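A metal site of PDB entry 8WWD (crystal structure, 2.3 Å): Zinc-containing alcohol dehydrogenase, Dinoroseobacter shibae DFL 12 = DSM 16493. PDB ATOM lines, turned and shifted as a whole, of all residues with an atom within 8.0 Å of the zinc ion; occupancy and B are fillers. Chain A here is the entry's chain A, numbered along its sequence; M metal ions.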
ATOM      1  N   VAL A  91     -15.486   0.605  14.992  1.00  0.00           N
ATOM      2  CA  VAL A  91     -14.461   1.525  14.424  1.00  0.00           C
ATOM      3  C   VAL A  91     -13.971   0.951  13.108  1.00  0.00           C
ATOM      4  O   VAL A  91     -13.508  -0.226  13.093  1.00  0.00           O
ATOM      5  CB  VAL A  91     -13.317   1.762  15.421  1.00  0.00           C
ATOM      6  CG1 VAL A  91     -12.264   2.706  14.846  1.00  0.00           C
ATOM      7  CG2 VAL A  91     -13.856   2.301  16.715  1.00  0.00           C
ATOM      8  N   THR A  92     -14.084   1.741  12.041  1.00  0.00           N
ATOM      9  CA  THR A  92     -13.824   1.326  10.642  1.00  0.00           C
ATOM     10  C   THR A  92     -12.702   2.184  10.056  1.00  0.00           C
ATOM     11  O   THR A  92     -12.469   3.315  10.546  1.00  0.00           O
ATOM     12  CB  THR A  92     -15.131   1.361   9.853  1.00  0.00           C
ATOM     13  OG1 THR A  92     -15.586   2.711   9.768  1.00  0.00           O
ATOM     14  CG2 THR A  92     -16.230   0.555  10.501  1.00  0.00           C
ATOM     15  N   CYS A  93     -11.991   1.681   9.053  1.00  0.00           N
ATOM     16  CA  CYS A  93     -10.739   2.302   8.554  1.00  0.00           C
ATOM     17  C   CYS A  93     -11.072   3.477   7.608  1.00  0.00           C
ATOM     18  O   CYS A  93     -10.221   4.394   7.476  1.00  0.00           O
ATOM     19  CB  CYS A  93      -9.847   1.245   7.909  1.00  0.00           C
ATOM     20  SG  CYS A  93     -10.256   0.880   6.227  1.00  0.00           S
ATOM     21  N   GLY A  94     -12.207   3.432   6.920  1.00  0.00           N
ATOM     22  CA  GLY A  94     -12.617   4.473   5.953  1.00  0.00           C
ATOM     23  C   GLY A  94     -11.948   4.382   4.565  1.00  0.00           C
ATOM     24  O   GLY A  94     -12.390   5.156   3.677  1.00  0.00           O
ATOM     25  N   THR A  95     -10.967   3.497   4.337  1.00  0.00           N
ATOM     26  CA  THR A  95     -10.202   3.460   3.047  1.00  0.00           C
ATOM     27  C   THR A  95     -10.115   2.074   2.390  1.00  0.00           C
ATOM     28  O   THR A  95      -9.526   2.031   1.299  1.00  0.00           O
ATOM     29  CB  THR A  95      -8.768   3.968   3.212  1.00  0.00           C
ATOM     30  OG1 THR A  95      -8.092   3.077   4.100  1.00  0.00           O
ATOM     31  CG2 THR A  95      -8.696   5.371   3.758  1.00  0.00           C
ATOM     32  N   CYS A  96     -10.682   1.016   2.979  1.00  0.00           N
ATOM     33  CA  CYS A  96     -10.708  -0.339   2.384  1.00  0.00           C
ATOM     34  C   CYS A  96     -11.822  -0.409   1.329  1.00  0.00           C
ATOM     35  O   CYS A  96     -12.672   0.473   1.236  1.00  0.00           O
ATOM     36  CB  CYS A  96     -10.832  -1.407   3.469  1.00  0.00           C
ATOM     37  SG  CYS A  96     -12.434  -1.551   4.195  1.00  0.00           S
ATOM     38  N   PRO A  97     -11.859  -1.441   0.465  1.00  0.00           N
ATOM     39  CA  PRO A  97     -12.938  -1.559  -0.523  1.00  0.00           C
ATOM     40  C   PRO A  97     -14.355  -1.560   0.076  1.00  0.00           C
ATOM     41  O   PRO A  97     -15.290  -1.020  -0.516  1.00  0.00           O
ATOM     42  CB  PRO A  97     -12.622  -2.900  -1.194  1.00  0.00           C
ATOM     43  CG  PRO A  97     -11.115  -3.036  -1.049  1.00  0.00           C
ATOM     44  CD  PRO A  97     -10.836  -2.490   0.341  1.00  0.00           C
ATOM     45  N   ALA A  98     -14.550  -2.219   1.199  1.00  0.00           N
ATOM     46  CA  ALA A  98     -15.890  -2.220   1.826  1.00  0.00           C
ATOM     47  C   ALA A  98     -16.237  -0.788   2.238  1.00  0.00           C
ATOM     48  O   ALA A  98     -17.339  -0.338   1.954  1.00  0.00           O
ATOM     49  CB  ALA A  98     -15.942  -3.234   2.946  1.00  0.00           C
ATOM     50  N   CYS A  99     -15.306  -0.054   2.846  1.00  0.00           N
ATOM     51  CA  CYS A  99     -15.551   1.319   3.363  1.00  0.00           C
ATOM     52  C   CYS A  99     -15.810   2.240   2.173  1.00  0.00           C
ATOM     53  O   CYS A  99     -16.817   2.977   2.185  1.00  0.00           O
ATOM     54  CB  CYS A  99     -14.402   1.798   4.244  1.00  0.00           C
ATOM     55  SG  CYS A  99     -14.308   0.970   5.832  1.00  0.00           S
ATOM     56  N   VAL A 100     -14.972   2.169   1.133  1.00  0.00           N
ATOM     57  CA  VAL A 100     -15.080   3.026  -0.076  1.00  0.00           C
ATOM     58  C   VAL A 100     -16.452   2.772  -0.728  1.00  0.00           C
ATOM     59  O   VAL A 100     -17.048   3.723  -1.222  1.00  0.00           O
ATOM     60  CB  VAL A 100     -13.913   2.774  -1.057  1.00  0.00           C
ATOM     61  CG1 VAL A 100     -14.235   3.200  -2.477  1.00  0.00           C
ATOM     62  CG2 VAL A 100     -12.626   3.432  -0.565  1.00  0.00           C
ATOM     63  N   ARG A 103     -20.070   0.375   2.710  1.00  0.00           N
ATOM     64  CA  ARG A 103     -20.436  -0.801   3.547  1.00  0.00           C
ATOM     65  C   ARG A 103     -19.378  -0.949   4.650  1.00  0.00           C
ATOM     66  O   ARG A 103     -18.880  -2.068   4.896  1.00  0.00           O
ATOM     67  CB  ARG A 103     -20.600  -2.020   2.657  1.00  0.00           C
ATOM     68  CG  ARG A 103     -21.751  -1.889   1.665  1.00  0.00           C
ATOM     69  CD  ARG A 103     -22.042  -3.188   0.941  1.00  0.00           C
ATOM     70  NE  ARG A 103     -22.768  -4.164   1.737  1.00  0.00           N
ATOM     71  CZ  ARG A 103     -23.042  -5.404   1.332  1.00  0.00           C
ATOM     72  NH1 ARG A 103     -22.693  -5.804   0.123  1.00  0.00           N
ATOM     73  NH2 ARG A 103     -23.699  -6.230   2.131  1.00  0.00           N
ATOM     74  N   ASP A 104     -19.092   0.144   5.352  1.00  0.00           N
ATOM     75  CA  ASP A 104     -18.023   0.209   6.381  1.00  0.00           C
ATOM     76  C   ASP A 104     -18.302  -0.784   7.524  1.00  0.00           C
ATOM     77  O   ASP A 104     -17.343  -1.139   8.203  1.00  0.00           O
ATOM     78  CB  ASP A 104     -17.849   1.640   6.850  1.00  0.00           C
ATOM     79  CG  ASP A 104     -19.173   2.299   7.156  1.00  0.00           C
ATOM     80  OD1 ASP A 104     -19.728   1.976   8.230  1.00  0.00           O
ATOM     81  OD2 ASP A 104     -19.649   3.111   6.313  1.00  0.00           O
ATOM     82  N   ASN A 105     -19.543  -1.262   7.693  1.00  0.00           N
ATOM     83  CA  ASN A 105     -19.868  -2.399   8.612  1.00  0.00           C
ATOM     84  C   ASN A 105     -19.054  -3.646   8.240  1.00  0.00           C
ATOM     85  O   ASN A 105     -18.896  -4.504   9.109  1.00  0.00           O
ATOM     86  CB  ASN A 105     -21.347  -2.746   8.603  1.00  0.00           C
ATOM     87  CG  ASN A 105     -21.853  -3.196   7.241  1.00  0.00           C
ATOM     88  OD1 ASN A 105     -21.483  -2.627   6.221  1.00  0.00           O
ATOM     89  ND2 ASN A 105     -22.692  -4.227   7.217  1.00  0.00           N
ATOM     90  N   LEU A 106     -18.574  -3.751   6.993  1.00  0.00           N
ATOM     91  CA  LEU A 106     -17.764  -4.891   6.477  1.00  0.00           C
ATOM     92  C   LEU A 106     -16.303  -4.496   6.328  1.00  0.00           C
ATOM     93  O   LEU A 106     -15.566  -5.233   5.645  1.00  0.00           O
ATOM     94  CB  LEU A 106     -18.345  -5.310   5.124  1.00  0.00           C
ATOM     95  CG  LEU A 106     -19.817  -5.730   5.187  1.00  0.00           C
ATOM     96  CD1 LEU A 106     -20.299  -6.170   3.809  1.00  0.00           C
ATOM     97  CD2 LEU A 106     -20.019  -6.813   6.225  1.00  0.00           C
ATOM     98  N   CYS A 107     -15.868  -3.407   6.964  1.00  0.00           N
ATOM     99  CA  CYS A 107     -14.457  -2.956   6.971  1.00  0.00           C
ATOM    100  C   CYS A 107     -13.541  -4.129   7.301  1.00  0.00           C
ATOM    101  O   CYS A 107     -13.769  -4.824   8.312  1.00  0.00           O
ATOM    102  CB  CYS A 107     -14.230  -1.831   7.980  1.00  0.00           C
ATOM    103  SG  CYS A 107     -12.496  -1.457   8.118  1.00  0.00           S
ATOM    104  N   ALA A 108     -12.489  -4.318   6.504  1.00  0.00           N
ATOM    105  CA  ALA A 108     -11.545  -5.455   6.642  1.00  0.00           C
ATOM    106  C   ALA A 108     -10.798  -5.372   7.975  1.00  0.00           C
ATOM    107  O   ALA A 108     -10.349  -6.412   8.424  1.00  0.00           O
ATOM    108  CB  ALA A 108     -10.601  -5.508   5.452  1.00  0.00           C
ATOM    109  N   THR A 109     -10.651  -4.188   8.596  1.00  0.00           N
ATOM    110  CA  THR A 109      -9.952  -4.064   9.913  1.00  0.00           C
ATOM    111  C   THR A 109     -10.916  -3.533  10.982  1.00  0.00           C
ATOM    112  O   THR A 109     -10.453  -2.972  11.970  1.00  0.00           O
ATOM    113  CB  THR A 109      -8.669  -3.242   9.783  1.00  0.00           C
ATOM    114  OG1 THR A 109      -9.047  -1.977   9.267  1.00  0.00           O
ATOM    115  CG2 THR A 109      -7.650  -3.880   8.865  1.00  0.00           C
ATOM    116  N   ARG A 110     -12.213  -3.810  10.849  1.00  0.00           N
ATOM    117  CA  ARG A 110     -13.238  -3.312  11.795  1.00  0.00           C
ATOM    118  C   ARG A 110     -12.895  -3.811  13.206  1.00  0.00           C
ATOM    119  O   ARG A 110     -12.551  -5.015  13.393  1.00  0.00           O
ATOM    120  CB  ARG A 110     -14.635  -3.740  11.367  1.00  0.00           C
ATOM    121  CG  ARG A 110     -14.857  -5.240  11.437  1.00  0.00           C
ATOM    122  CD  ARG A 110     -16.192  -5.621  10.836  1.00  0.00           C
ATOM    123  NE  ARG A 110     -16.547  -6.989  11.199  1.00  0.00           N
ATOM    124  CZ  ARG A 110     -17.321  -7.799  10.490  1.00  0.00           C
ATOM    125  NH1 ARG A 110     -17.858  -7.373   9.350  1.00  0.00           N
ATOM    126  NH2 ARG A 110     -17.561  -9.024  10.917  1.00  0.00           N
HETATM  127 ZN    ZN M   1     -12.293  -0.250   6.121  1.00  0.00          ZN
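SG of Cys 96 lies close to N of Ala 108 (3.6 Å).
N of Ala 98 sits close to SG of Cys 96 (3.7 Å).
The side-chain sulfur (SG) of Cys 93 sits close to the backbone NH (N) of Thr 95 (3.3 Å).
SG of Cys 107 lies close to N of Thr 109, at 3.3 Å.
The side-chain sulfur (SG) of Cys 107 lies close to the backbone NH (N) of Arg 110 (3.6 Å).
SG of Cys 99 lies close to N of Gly 94 (3.4 Å).
The zinc ion is bound by the side-chain sulfur (SG) of Cys 96 (2.3 Å), the side-chain sulfur (SG) of Cys 93 (2.3 Å), the side-chain sulfur (SG) of Cys 107 (2.3 Å) and the side-chain sulfur (SG) of Cys 99 (2.4 Å).
Merely in contact with the zinc ion: Gly 94 (3.8 Å).
Five residues have an atom within 4 Å of the zinc ion: Cys 93, Gly 94, Cys 96, Cys 99 and Cys 107.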
